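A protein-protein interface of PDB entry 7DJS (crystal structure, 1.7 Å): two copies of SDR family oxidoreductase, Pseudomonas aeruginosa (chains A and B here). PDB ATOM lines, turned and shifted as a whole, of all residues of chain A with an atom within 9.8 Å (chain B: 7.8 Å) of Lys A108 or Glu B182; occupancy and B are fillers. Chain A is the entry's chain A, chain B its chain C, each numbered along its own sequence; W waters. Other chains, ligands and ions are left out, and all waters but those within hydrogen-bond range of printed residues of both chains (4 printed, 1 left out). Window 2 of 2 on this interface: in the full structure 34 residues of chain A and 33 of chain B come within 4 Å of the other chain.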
ATOM      1  N   GLU A 103      12.294   0.848 -11.354  1.00  0.00           N
ATOM      2  CA  GLU A 103      12.706  -0.488 -11.780  1.00  0.00           C
ATOM      3  C   GLU A 103      14.218  -0.420 -11.937  1.00  0.00           C
ATOM      4  O   GLU A 103      14.702   0.257 -12.847  1.00  0.00           O
ATOM      5  CB  GLU A 103      12.018  -0.883 -13.087  1.00  0.00           C
ATOM      6  CG  GLU A 103      12.064  -2.376 -13.383  1.00  0.00           C
ATOM      7  CD  GLU A 103      13.397  -2.799 -13.977  1.00  0.00           C
ATOM      8  OE1 GLU A 103      13.704  -2.358 -15.107  1.00  0.00           O
ATOM      9  OE2 GLU A 103      14.141  -3.553 -13.310  1.00  0.00           O
ATOM     10  N   GLU A 105      16.595  -3.216 -10.687  1.00  0.00           N
ATOM     11  CA  GLU A 105      17.340  -4.447 -10.445  1.00  0.00           C
ATOM     12  C   GLU A 105      18.240  -4.809 -11.615  1.00  0.00           C
ATOM     13  O   GLU A 105      17.948  -4.510 -12.774  1.00  0.00           O
ATOM     14  CB  GLU A 105      16.397  -5.613 -10.206  1.00  0.00           C
ATOM     15  CG  GLU A 105      15.819  -5.651  -8.851  1.00  0.00           C
ATOM     16  CD  GLU A 105      14.659  -6.596  -8.834  1.00  0.00           C
ATOM     17  OE1 GLU A 105      14.851  -7.759  -8.417  1.00  0.00           O
ATOM     18  OE2 GLU A 105      13.571  -6.177  -9.274  1.00  0.00           O
ATOM     19  N   GLN A 106      19.325  -5.516 -11.306  1.00  0.00           N
ATOM     20  CA  GLN A 106      20.258  -5.936 -12.339  1.00  0.00           C
ATOM     21  C   GLN A 106      20.578  -7.424 -12.323  1.00  0.00           C
ATOM     22  O   GLN A 106      21.388  -7.867 -13.147  1.00  0.00           O
ATOM     23  CB  GLN A 106      21.563  -5.131 -12.232  1.00  0.00           C
ATOM     24  CG  GLN A 106      21.447  -3.713 -12.786  1.00  0.00           C
ATOM     25  CD  GLN A 106      21.447  -3.675 -14.311  1.00  0.00           C
ATOM     26  OE1 GLN A 106      20.393  -3.583 -14.946  1.00  0.00           O
ATOM     27  NE2 GLN A 106      22.636  -3.737 -14.902  1.00  0.00           N
ATOM     28  N   GLY A 107      19.974  -8.212 -11.434  1.00  0.00           N
ATOM     29  CA  GLY A 107      20.316  -9.618 -11.371  1.00  0.00           C
ATOM     30  C   GLY A 107      19.176 -10.497 -10.906  1.00  0.00           C
ATOM     31  O   GLY A 107      18.111 -10.021 -10.504  1.00  0.00           O
ATOM     32  N   LYS A 108      19.422 -11.807 -10.971  1.00  0.00           N
ATOM     33  CA  LYS A 108      18.512 -12.784 -10.392  1.00  0.00           C
ATOM     34  C   LYS A 108      18.399 -12.568  -8.882  1.00  0.00           C
ATOM     35  O   LYS A 108      19.189 -11.836  -8.271  1.00  0.00           O
ATOM     36  CB  LYS A 108      18.986 -14.203 -10.701  1.00  0.00           C
ATOM     37  CG  LYS A 108      18.935 -14.543 -12.191  1.00  0.00           C
ATOM     38  CD  LYS A 108      19.385 -15.976 -12.462  1.00  0.00           C
ATOM     39  CE  LYS A 108      19.492 -16.231 -13.960  1.00  0.00           C
ATOM     40  NZ  LYS A 108      19.759 -17.667 -14.273  1.00  0.00           N
ATOM     41  N   LEU A 109      17.399 -13.222  -8.279  1.00  0.00           N
ATOM     42  CA  LEU A 109      17.056 -12.930  -6.885  1.00  0.00           C
ATOM     43  C   LEU A 109      18.277 -12.997  -5.976  1.00  0.00           C
ATOM     44  O   LEU A 109      18.527 -12.078  -5.187  1.00  0.00           O
ATOM     45  CB  LEU A 109      15.968 -13.880  -6.372  1.00  0.00           C
ATOM     46  CG  LEU A 109      15.361 -13.478  -5.010  1.00  0.00           C
ATOM     47  CD1 LEU A 109      13.888 -13.904  -4.880  1.00  0.00           C
ATOM     48  CD2 LEU A 109      16.151 -14.042  -3.811  1.00  0.00           C
ATOM     49  N   ALA A 110      19.059 -14.078  -6.072  1.00  0.00           N
ATOM     50  CA  ALA A 110      20.158 -14.245  -5.130  1.00  0.00           C
ATOM     51  C   ALA A 110      21.272 -13.234  -5.351  1.00  0.00           C
ATOM     52  O   ALA A 110      22.167 -13.132  -4.503  1.00  0.00           O
ATOM     53  CB  ALA A 110      20.726 -15.663  -5.216  1.00  0.00           C
ATOM     54  N   ASP A 111      21.236 -12.491  -6.452  1.00  0.00           N
ATOM     55  CA  ASP A 111      22.263 -11.515  -6.773  1.00  0.00           C
ATOM     56  C   ASP A 111      21.876 -10.082  -6.439  1.00  0.00           C
ATOM     57  O   ASP A 111      22.717  -9.191  -6.569  1.00  0.00           O
ATOM     58  CB  ASP A 111      22.653 -11.636  -8.246  1.00  0.00           C
ATOM     59  CG  ASP A 111      23.248 -12.990  -8.568  1.00  0.00           C
ATOM     60  OD1 ASP A 111      23.895 -13.577  -7.673  1.00  0.00           O
ATOM     61  OD2 ASP A 111      23.067 -13.467  -9.702  1.00  0.00           O
ATOM     62  N   GLY A 112      20.654  -9.843  -5.976  1.00  0.00           N
ATOM     63  CA  GLY A 112      20.240  -8.510  -5.591  1.00  0.00           C
ATOM     64  C   GLY A 112      20.830  -8.088  -4.265  1.00  0.00           C
ATOM     65  O   GLY A 112      21.515  -8.846  -3.579  1.00  0.00           O
ATOM     66  N   ASN A 113      20.565  -6.841  -3.893  1.00  0.00           N
ATOM     67  CA  ASN A 113      21.042  -6.343  -2.614  1.00  0.00           C
ATOM     68  C   ASN A 113      19.926  -5.627  -1.867  1.00  0.00           C
ATOM     69  O   ASN A 113      18.895  -5.249  -2.438  1.00  0.00           O
ATOM     70  CB  ASN A 113      22.281  -5.431  -2.772  1.00  0.00           C
ATOM     71  CG  ASN A 113      22.000  -4.170  -3.558  1.00  0.00           C
ATOM     72  OD1 ASN A 113      21.250  -3.296  -3.114  1.00  0.00           O
ATOM     73  ND2 ASN A 113      22.626  -4.050  -4.727  1.00  0.00           N
ATOM     74  N   GLU A 116      18.658  -2.126  -2.985  1.00  0.00           N
ATOM     75  CA  GLU A 116      17.704  -2.205  -4.086  1.00  0.00           C
ATOM     76  C   GLU A 116      16.337  -2.645  -3.588  1.00  0.00           C
ATOM     77  O   GLU A 116      15.311  -2.093  -4.006  1.00  0.00           O
ATOM     78  CB  GLU A 116      18.188  -3.183  -5.155  1.00  0.00           C
ATOM     79  CG  GLU A 116      19.452  -2.792  -5.889  1.00  0.00           C
ATOM     80  CD  GLU A 116      19.927  -3.917  -6.804  1.00  0.00           C
ATOM     81  OE1 GLU A 116      19.771  -5.107  -6.430  1.00  0.00           O
ATOM     82  OE2 GLU A 116      20.443  -3.615  -7.894  1.00  0.00           O
ATOM     83  N   ALA A 158       5.730 -14.146 -13.216  1.00  0.00           N
ATOM     84  CA  ALA A 158       7.158 -13.996 -12.956  1.00  0.00           C
ATOM     85  C   ALA A 158       7.752 -12.833 -13.743  1.00  0.00           C
ATOM     86  O   ALA A 158       7.308 -12.504 -14.842  1.00  0.00           O
ATOM     87  CB  ALA A 158       7.894 -15.278 -13.334  1.00  0.00           C
ATOM     88  N   ALA A 159       8.808 -12.236 -13.191  1.00  0.00           N
ATOM     89  CA  ALA A 159       9.621 -11.266 -13.922  1.00  0.00           C
ATOM     90  C   ALA A 159      11.078 -11.627 -13.684  1.00  0.00           C
ATOM     91  O   ALA A 159      11.717 -11.096 -12.769  1.00  0.00           O
ATOM     92  CB  ALA A 159       9.333  -9.832 -13.477  1.00  0.00           C
ATOM     93  N   PRO A 160      11.637 -12.531 -14.492  1.00  0.00           N
ATOM     94  CA  PRO A 160      13.028 -12.955 -14.279  1.00  0.00           C
ATOM     95  C   PRO A 160      13.988 -11.778 -14.339  1.00  0.00           C
ATOM     96  O   PRO A 160      13.863 -10.892 -15.191  1.00  0.00           O
ATOM     97  CB  PRO A 160      13.289 -13.931 -15.433  1.00  0.00           C
ATOM     98  CG  PRO A 160      11.980 -14.272 -15.990  1.00  0.00           C
ATOM     99  CD  PRO A 160      11.010 -13.183 -15.649  1.00  0.00           C
ATOM    100  N   LYS A 161      14.957 -11.783 -13.422  1.00  0.00           N
ATOM    101  CA  LYS A 161      15.924 -10.710 -13.209  1.00  0.00           C
ATOM    102  C   LYS A 161      15.268  -9.426 -12.726  1.00  0.00           C
ATOM    103  O   LYS A 161      15.917  -8.371 -12.710  1.00  0.00           O
ATOM    104  CB  LYS A 161      16.767 -10.431 -14.466  1.00  0.00           C
ATOM    105  CG  LYS A 161      17.808 -11.509 -14.731  1.00  0.00           C
ATOM    106  CD  LYS A 161      18.803 -11.078 -15.796  1.00  0.00           C
ATOM    107  CE  LYS A 161      19.950 -12.070 -15.899  1.00  0.00           C
ATOM    108  NZ  LYS A 161      19.874 -12.869 -17.156  1.00  0.00           N
ATOM    109  N   MET A 162      13.999  -9.495 -12.320  1.00  0.00           N
ATOM    110  CA  MET A 162      13.287  -8.372 -11.717  1.00  0.00           C
ATOM    111  C   MET A 162      12.371  -8.885 -10.616  1.00  0.00           C
ATOM    112  O   MET A 162      11.200  -8.489 -10.523  1.00  0.00           O
ATOM    113  CB  MET A 162      12.477  -7.597 -12.757  1.00  0.00           C
ATOM    114  CG  MET A 162      13.305  -6.901 -13.834  1.00  0.00           C
ATOM    115  SD  MET A 162      12.268  -6.093 -15.080  1.00  0.00           S
ATOM    116  CE  MET A 162      11.345  -7.465 -15.759  1.00  0.00           C
ATOM    117  N   SER A 163      12.894  -9.788  -9.772  1.00  0.00           N
ATOM    118  CA  SER A 163      12.060 -10.463  -8.783  1.00  0.00           C
ATOM    119  C   SER A 163      11.529  -9.492  -7.736  1.00  0.00           C
ATOM    120  O   SER A 163      10.400  -9.652  -7.260  1.00  0.00           O
ATOM    121  CB  SER A 163      12.831 -11.589  -8.084  1.00  0.00           C
ATOM    122  OG  SER A 163      13.974 -11.093  -7.396  1.00  0.00           O
ATOM    123  N   ILE A 164      12.342  -8.517  -7.318  1.00  0.00           N
ATOM    124  CA  ILE A 164      11.842  -7.551  -6.338  1.00  0.00           C
ATOM    125  C   ILE A 164      10.752  -6.697  -6.961  1.00  0.00           C
ATOM    126  O   ILE A 164       9.720  -6.422  -6.333  1.00  0.00           O
ATOM    127  CB  ILE A 164      12.979  -6.671  -5.786  1.00  0.00           C
ATOM    128  CG1 ILE A 164      14.094  -7.541  -5.206  1.00  0.00           C
ATOM    129  CG2 ILE A 164      12.435  -5.726  -4.705  1.00  0.00           C
ATOM    130  CD1 ILE A 164      15.379  -6.773  -4.969  1.00  0.00           C
ATOM    131  N   TYR A 165      10.981  -6.244  -8.192  1.00  0.00           N
ATOM    132  CA  TYR A 165       9.965  -5.496  -8.926  1.00  0.00           C
ATOM    133  C   TYR A 165       8.666  -6.288  -9.026  1.00  0.00           C
ATOM    134  O   TYR A 165       7.572  -5.756  -8.791  1.00  0.00           O
ATOM    135  CB  TYR A 165      10.508  -5.163 -10.315  1.00  0.00           C
ATOM    136  CG  TYR A 165       9.595  -4.305 -11.145  1.00  0.00           C
ATOM    137  CD1 TYR A 165       9.526  -2.938 -10.935  1.00  0.00           C
ATOM    138  CD2 TYR A 165       8.823  -4.861 -12.158  1.00  0.00           C
ATOM    139  CE1 TYR A 165       8.711  -2.143 -11.713  1.00  0.00           C
ATOM    140  CE2 TYR A 165       7.997  -4.073 -12.939  1.00  0.00           C
ATOM    141  CZ  TYR A 165       7.947  -2.720 -12.706  1.00  0.00           C
ATOM    142  OH  TYR A 165       7.130  -1.927 -13.476  1.00  0.00           O
ATOM    143  N   ALA A 166       8.763  -7.572  -9.371  1.00  0.00           N
ATOM    144  CA  ALA A 166       7.557  -8.387  -9.459  1.00  0.00           C
ATOM    145  C   ALA A 166       6.868  -8.489  -8.105  1.00  0.00           C
ATOM    146  O   ALA A 166       5.637  -8.380  -8.022  1.00  0.00           O
ATOM    147  CB  ALA A 166       7.898  -9.774 -10.008  1.00  0.00           C
ATOM    148  N   ALA A 167       7.642  -8.709  -7.035  1.00  0.00           N
ATOM    149  CA  ALA A 167       7.046  -8.731  -5.704  1.00  0.00           C
ATOM    150  C   ALA A 167       6.302  -7.427  -5.434  1.00  0.00           C
ATOM    151  O   ALA A 167       5.174  -7.438  -4.923  1.00  0.00           O
ATOM    152  CB  ALA A 167       8.124  -8.963  -4.643  1.00  0.00           C
ATOM    153  N   TRP B 129      12.443 -12.924   1.096  1.00  0.00           N
ATOM    154  CA  TRP B 129      13.460 -12.559   0.124  1.00  0.00           C
ATOM    155  C   TRP B 129      14.857 -12.867   0.655  1.00  0.00           C
ATOM    156  O   TRP B 129      15.673 -13.487  -0.040  1.00  0.00           O
ATOM    157  CB  TRP B 129      13.315 -11.078  -0.225  1.00  0.00           C
ATOM    158  CG  TRP B 129      14.364 -10.554  -1.140  1.00  0.00           C
ATOM    159  CD1 TRP B 129      14.430 -10.699  -2.497  1.00  0.00           C
ATOM    160  CD2 TRP B 129      15.504  -9.774  -0.763  1.00  0.00           C
ATOM    161  NE1 TRP B 129      15.542 -10.045  -2.989  1.00  0.00           N
ATOM    162  CE2 TRP B 129      16.219  -9.480  -1.938  1.00  0.00           C
ATOM    163  CE3 TRP B 129      15.981  -9.287   0.459  1.00  0.00           C
ATOM    164  CZ2 TRP B 129      17.397  -8.727  -1.931  1.00  0.00           C
ATOM    165  CZ3 TRP B 129      17.155  -8.533   0.465  1.00  0.00           C
ATOM    166  CH2 TRP B 129      17.844  -8.264  -0.720  1.00  0.00           C
ATOM    167  N   LYS B 133      17.415 -15.543  -0.766  1.00  0.00           N
ATOM    168  CA  LYS B 133      18.679 -14.978  -1.236  1.00  0.00           C
ATOM    169  C   LYS B 133      19.868 -15.780  -0.726  1.00  0.00           C
ATOM    170  O   LYS B 133      20.863 -15.954  -1.441  1.00  0.00           O
ATOM    171  CB  LYS B 133      18.778 -13.519  -0.785  1.00  0.00           C
ATOM    172  CG  LYS B 133      20.033 -12.775  -1.169  1.00  0.00           C
ATOM    173  CD  LYS B 133      19.910 -11.319  -0.710  1.00  0.00           C
ATOM    174  CE  LYS B 133      21.118 -10.506  -1.101  1.00  0.00           C
ATOM    175  NZ  LYS B 133      22.381 -11.171  -0.697  1.00  0.00           N
ATOM    176  N   ILE B 136      19.491 -20.025  -1.912  1.00  0.00           N
ATOM    177  CA  ILE B 136      19.696 -20.420  -3.307  1.00  0.00           C
ATOM    178  C   ILE B 136      21.161 -20.736  -3.608  1.00  0.00           C
ATOM    179  O   ILE B 136      21.425 -21.758  -4.255  1.00  0.00           O
ATOM    180  CB  ILE B 136      19.083 -19.381  -4.247  1.00  0.00           C
ATOM    181  CG1 ILE B 136      17.550 -19.485  -4.200  1.00  0.00           C
ATOM    182  CG2 ILE B 136      19.588 -19.543  -5.683  1.00  0.00           C
ATOM    183  CD1 ILE B 136      16.826 -18.342  -4.904  1.00  0.00           C
ATOM    184  N   LEU B 140      22.348 -24.174  -5.099  1.00  0.00           N
ATOM    185  CA  LEU B 140      23.045 -24.207  -6.382  1.00  0.00           C
ATOM    186  C   LEU B 140      24.308 -25.049  -6.288  1.00  0.00           C
ATOM    187  O   LEU B 140      24.610 -25.837  -7.194  1.00  0.00           O
ATOM    188  CB  LEU B 140      23.395 -22.790  -6.829  1.00  0.00           C
ATOM    189  CG  LEU B 140      22.279 -21.886  -7.363  1.00  0.00           C
ATOM    190  CD1 LEU B 140      22.826 -20.507  -7.669  1.00  0.00           C
ATOM    191  CD2 LEU B 140      21.648 -22.503  -8.595  1.00  0.00           C
ATOM    192  N   LEU B 175       7.730 -13.047  -5.608  1.00  0.00           N
ATOM    193  CA  LEU B 175       9.075 -13.576  -5.390  1.00  0.00           C
ATOM    194  C   LEU B 175       9.153 -15.036  -5.798  1.00  0.00           C
ATOM    195  O   LEU B 175      10.123 -15.466  -6.437  1.00  0.00           O
ATOM    196  CB  LEU B 175       9.469 -13.451  -3.917  1.00  0.00           C
ATOM    197  CG  LEU B 175       9.697 -12.051  -3.342  1.00  0.00           C
ATOM    198  CD1 LEU B 175       9.967 -12.115  -1.846  1.00  0.00           C
ATOM    199  CD2 LEU B 175      10.836 -11.366  -4.043  1.00  0.00           C
ATOM    200  N   THR B 176       8.137 -15.809  -5.417  1.00  0.00           N
ATOM    201  CA  THR B 176       8.103 -17.242  -5.698  1.00  0.00           C
ATOM    202  C   THR B 176       8.154 -17.511  -7.195  1.00  0.00           C
ATOM    203  O   THR B 176       8.986 -18.296  -7.673  1.00  0.00           O
ATOM    204  CB  THR B 176       6.833 -17.839  -5.093  1.00  0.00           C
ATOM    205  OG1 THR B 176       6.857 -17.681  -3.671  1.00  0.00           O
ATOM    206  CG2 THR B 176       6.710 -19.315  -5.439  1.00  0.00           C
ATOM    207  N   LYS B 177       7.248 -16.893  -7.952  1.00  0.00           N
ATOM    208  CA  LYS B 177       7.208 -17.154  -9.384  1.00  0.00           C
ATOM    209  C   LYS B 177       8.475 -16.664 -10.071  1.00  0.00           C
ATOM    210  O   LYS B 177       8.975 -17.322 -10.983  1.00  0.00           O
ATOM    211  CB  LYS B 177       5.970 -16.507 -10.007  1.00  0.00           C
ATOM    212  CG  LYS B 177       4.690 -17.243  -9.625  1.00  0.00           C
ATOM    213  CD  LYS B 177       3.462 -16.581 -10.208  1.00  0.00           C
ATOM    214  CE  LYS B 177       2.193 -17.357  -9.889  1.00  0.00           C
ATOM    215  NZ  LYS B 177       1.035 -16.723 -10.591  1.00  0.00           N
ATOM    216  N   SER B 178       8.995 -15.500  -9.669  1.00  0.00           N
ATOM    217  CA  SER B 178      10.173 -14.971 -10.346  1.00  0.00           C
ATOM    218  C   SER B 178      11.376 -15.872 -10.109  1.00  0.00           C
ATOM    219  O   SER B 178      12.080 -16.245 -11.054  1.00  0.00           O
ATOM    220  CB  SER B 178      10.453 -13.536  -9.885  1.00  0.00           C
ATOM    221  OG  SER B 178       9.382 -12.669 -10.261  1.00  0.00           O
ATOM    222  N   ALA B 179      11.607 -16.256  -8.854  1.00  0.00           N
ATOM    223  CA  ALA B 179      12.726 -17.153  -8.559  1.00  0.00           C
ATOM    224  C   ALA B 179      12.551 -18.503  -9.247  1.00  0.00           C
ATOM    225  O   ALA B 179      13.531 -19.101  -9.708  1.00  0.00           O
ATOM    226  CB  ALA B 179      12.872 -17.339  -7.046  1.00  0.00           C
ATOM    227  N   ALA B 180      11.311 -19.002  -9.323  1.00  0.00           N
ATOM    228  CA  ALA B 180      11.079 -20.279 -10.003  1.00  0.00           C
ATOM    229  C   ALA B 180      11.564 -20.232 -11.447  1.00  0.00           C
ATOM    230  O   ALA B 180      12.211 -21.174 -11.926  1.00  0.00           O
ATOM    231  CB  ALA B 180       9.596 -20.647  -9.953  1.00  0.00           C
ATOM    232  N   ILE B 181      11.265 -19.144 -12.156  1.00  0.00           N
ATOM    233  CA  ILE B 181      11.678 -19.039 -13.550  1.00  0.00           C
ATOM    234  C   ILE B 181      13.183 -18.815 -13.643  1.00  0.00           C
ATOM    235  O   ILE B 181      13.856 -19.401 -14.503  1.00  0.00           O
ATOM    236  CB  ILE B 181      10.893 -17.921 -14.263  1.00  0.00           C
ATOM    237  CG1 ILE B 181       9.400 -18.240 -14.275  1.00  0.00           C
ATOM    238  CG2 ILE B 181      11.403 -17.730 -15.683  1.00  0.00           C
ATOM    239  CD1 ILE B 181       9.060 -19.616 -14.783  1.00  0.00           C
ATOM    240  N   GLU B 182      13.736 -17.983 -12.749  1.00  0.00           N
ATOM    241  CA  GLU B 182      15.157 -17.646 -12.818  1.00  0.00           C
ATOM    242  C   GLU B 182      16.041 -18.873 -12.646  1.00  0.00           C
ATOM    243  O   GLU B 182      17.094 -18.981 -13.290  1.00  0.00           O
ATOM    244  CB  GLU B 182      15.497 -16.607 -11.750  1.00  0.00           C
ATOM    245  CG  GLU B 182      14.967 -15.211 -12.054  1.00  0.00           C
ATOM    246  CD  GLU B 182      15.201 -14.248 -10.902  1.00  0.00           C
ATOM    247  OE1 GLU B 182      15.597 -14.708  -9.815  1.00  0.00           O
ATOM    248  OE2 GLU B 182      14.984 -13.034 -11.084  1.00  0.00           O
ATOM    249  N   TYR B 183      15.640 -19.804 -11.781  1.00  0.00           N
ATOM    250  CA  TYR B 183      16.494 -20.931 -11.408  1.00  0.00           C
ATOM    251  C   TYR B 183      15.937 -22.265 -11.890  1.00  0.00           C
ATOM    252  O   TYR B 183      16.382 -23.324 -11.425  1.00  0.00           O
ATOM    253  CB  TYR B 183      16.704 -20.939  -9.891  1.00  0.00           C
ATOM    254  CG  TYR B 183      17.442 -19.707  -9.420  1.00  0.00           C
ATOM    255  CD1 TYR B 183      18.823 -19.609  -9.545  1.00  0.00           C
ATOM    256  CD2 TYR B 183      16.754 -18.627  -8.874  1.00  0.00           C
ATOM    257  CE1 TYR B 183      19.505 -18.471  -9.133  1.00  0.00           C
ATOM    258  CE2 TYR B 183      17.426 -17.480  -8.456  1.00  0.00           C
ATOM    259  CZ  TYR B 183      18.800 -17.410  -8.587  1.00  0.00           C
ATOM    260  OH  TYR B 183      19.473 -16.285  -8.166  1.00  0.00           O
ATOM    261  N   ALA B 184      14.991 -22.228 -12.836  1.00  0.00           N
ATOM    262  CA  ALA B 184      14.324 -23.446 -13.290  1.00  0.00           C
ATOM    263  C   ALA B 184      15.312 -24.428 -13.907  1.00  0.00           C
ATOM    264  O   ALA B 184      15.192 -25.643 -13.716  1.00  0.00           O
ATOM    265  CB  ALA B 184      13.234 -23.096 -14.301  1.00  0.00           C
ATOM    266  N   LYS B 185      16.279 -23.931 -14.659  1.00  0.00           N
ATOM    267  CA  LYS B 185      17.238 -24.823 -15.297  1.00  0.00           C
ATOM    268  C   LYS B 185      18.444 -25.103 -14.422  1.00  0.00           C
ATOM    269  O   LYS B 185      19.390 -25.749 -14.887  1.00  0.00           O
ATOM    270  CB  LYS B 185      17.671 -24.246 -16.641  1.00  0.00           C
ATOM    271  CG  LYS B 185      16.559 -24.315 -17.677  1.00  0.00           C
ATOM    272  CD  LYS B 185      17.020 -23.835 -19.036  1.00  0.00           C
ATOM    273  CE  LYS B 185      15.855 -23.669 -20.003  1.00  0.00           C
ATOM    274  NZ  LYS B 185      14.873 -22.640 -19.538  1.00  0.00           N
ATOM    275  N   LYS B 186      18.427 -24.644 -13.169  1.00  0.00           N
ATOM    276  CA  LYS B 186      19.525 -24.857 -12.238  1.00  0.00           C
ATOM    277  C   LYS B 186      19.148 -25.808 -11.108  1.00  0.00           C
ATOM    278  O   LYS B 186      19.873 -25.902 -10.113  1.00  0.00           O
ATOM    279  CB  LYS B 186      20.010 -23.513 -11.686  1.00  0.00           C
ATOM    280  CG  LYS B 186      20.645 -22.619 -12.747  1.00  0.00           C
ATOM    281  CD  LYS B 186      22.057 -22.184 -12.356  1.00  0.00           C
ATOM    282  CE  LYS B 186      22.416 -20.822 -12.954  1.00  0.00           C
ATOM    283  NZ  LYS B 186      22.543 -19.761 -11.905  1.00  0.00           N
ATOM    284  N   ILE B 188      16.525 -25.820  -9.005  1.00  0.00           N
ATOM    285  CA  ILE B 188      15.810 -25.283  -7.855  1.00  0.00           C
ATOM    286  C   ILE B 188      14.359 -25.081  -8.264  1.00  0.00           C
ATOM    287  O   ILE B 188      14.080 -24.360  -9.229  1.00  0.00           O
ATOM    288  CB  ILE B 188      16.424 -23.968  -7.361  1.00  0.00           C
ATOM    289  CG1 ILE B 188      17.906 -24.161  -7.029  1.00  0.00           C
ATOM    290  CG2 ILE B 188      15.677 -23.463  -6.119  1.00  0.00           C
ATOM    291  CD1 ILE B 188      18.598 -22.892  -6.593  1.00  0.00           C
ATOM    292  N   VAL B 190      10.655 -23.628  -6.882  1.00  0.00           N
ATOM    293  CA  VAL B 190      10.177 -22.627  -5.935  1.00  0.00           C
ATOM    294  C   VAL B 190       8.663 -22.571  -6.076  1.00  0.00           C
ATOM    295  O   VAL B 190       8.157 -22.310  -7.171  1.00  0.00           O
ATOM    296  CB  VAL B 190      10.781 -21.233  -6.188  1.00  0.00           C
ATOM    297  CG1 VAL B 190      10.394 -20.287  -5.060  1.00  0.00           C
ATOM    298  CG2 VAL B 190      12.310 -21.310  -6.329  1.00  0.00           C
HETATM  299  O   HOH W   1      17.126  -9.722  -5.329  1.00  0.00           O
HETATM  300  O   HOH W   2      23.070 -14.408  -2.021  1.00  0.00           O
HETATM  301  O   HOH W   3      24.163  -8.504  -1.431  1.00  0.00           O
HETATM  302  O   HOH W   4      22.035 -16.234  -8.804  1.00  0.00           O
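The side-chain carboxylate (OE2) of Glu B182 lies within hydrogen-bond range of the backbone NH (N) of Lys A161, at 2.7 Å. N of Ala A159 sits at hydrogen-bond distance from OG of Ser B178 (3.0 Å). The backbone carbonyl oxygen (O) of Glu B182 is in hydrogen-bond range of the side-chain amino group (NZ) of Lys A108, 3.1 Å away. N of Ala A110 sits at hydrogen-bond distance from OH of Tyr B183. OE1 of Glu B182 lies within hydrogen-bond range of N of Leu A109, at 2.8 Å.
Water W4 bridges OH of Tyr B183 (2.6 Å) and OD2 of Asp A111 (3.1 Å). Water W1 bridges O of Leu A109 (2.7 Å) and NE1 of Trp B129 (2.8 Å). Water W2 bridges the backbone carbonyl oxygen of Lys B133 (2.8 Å) and the backbone carbonyl oxygen of Ala A110 (2.9 Å). Water W3 bridges the side-chain amino group of Lys B133 (3.3 Å) and the backbone carbonyl oxygen of Gly A112 (3.4 Å).
No position is printed for both chains. Of the 24 pairs that touch across the chains among the printed residues, none has its exchanged pair printed and touching as well.
The side-chain carboxylate of Glu A105 is in hydrogen-bond range of the backbone NH of Ile A164 (2.8 Å). OD1 of Asn A113 sits at hydrogen-bond distance from N of Glu A116 (2.8 Å). O of Tyr B183 sits at hydrogen-bond distance from N of Ile B188 (3.5 Å). The side-chain carboxylate (OE1) of Glu A105 is in hydrogen-bond range of the backbone NH (N) of Ser A163, at 3.1 Å.
Leu A109 touches Tyr B183 (N to OH, 3.7 Å). Trp B129 touches Asn A113 (CH2 to C, 3.6 Å). Ala A158 touches Lys B177 (CB to O, 3.3 Å). Ser B178 touches Ala A158 (OG to CA, 3.7 Å). Ile B181 touches Ala A158. Pro A160 touches Glu B182 (C to OE2, 3.6 Å). N of Met A162 touches OE2 of Glu B182, at 3.9 Å. Leu B175 touches Ser A163. Ser B178 touches Ser A163 (CB to CB, 3.6 Å). OG of Ser B178 touches CB of Ala A166, 3.3 Å away.
Of the 18 printed residues of chain B, 8 touch a printed residue of chain A. Hydrophobic or aromatic side chains of chain B within 4 Å of the printed part of chain A: Trp B129, Leu B175, Ile B181 and Tyr B183. Of the 21 printed residues of chain A, 14 touch a printed residue of chain B. Hydrophobic or aromatic side chains of chain A within 4 Å of the printed part of chain B: Leu A109, Ala A110, Ala A158, Pro A160, Ile A164, Ala A166 and Ala A167. Along chain A the printed residues that touch a printed residue of chain B span positions 108 to 167. Among the printed residues, no Asp or Glu carboxylate lies within 4 Å of a Lys or Arg side-chain nitrogen of the other chain.
No residue of chain B comes within 4 Å of Gly A107. Of chain B, only Glu B182 (3.1 Å) and Tyr B183 (3.3 Å) come within 4 Å of Lys A108. Printed residues of chain B within 4 Å of Leu A109: Trp B129 (3.8 Å), Lys B133 (3.6 Å), Glu B182 (2.8 Å) and Tyr B183 (3.7 Å). Of the printed residues of chain B, Asn A113 touches Trp B129 (3.6 Å). Of the printed residues of chain B, Ser A163 touches Leu B175 (3.7 Å), Ser B178 (3.6 Å) and Glu B182 (3.97 Å). Printed residues of chain B within 4 Å of Ile A164: Trp B129 (3.6 Å). Of the printed residues of chain B, Ala A167 touches Leu B175 (3.7 Å). Thr B176 touches none of the printed residues of chain A. Ala B179 touches none of the printed residues of chain A. Tyr B183 touches just these residues of chain A: Lys A108 (3.3 Å), Leu A109 (3.7 Å) and Ala A110 (3.1 Å). The nearest residue of chain B that does not touch Lys A108 is Lys B186 (4.2 Å).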
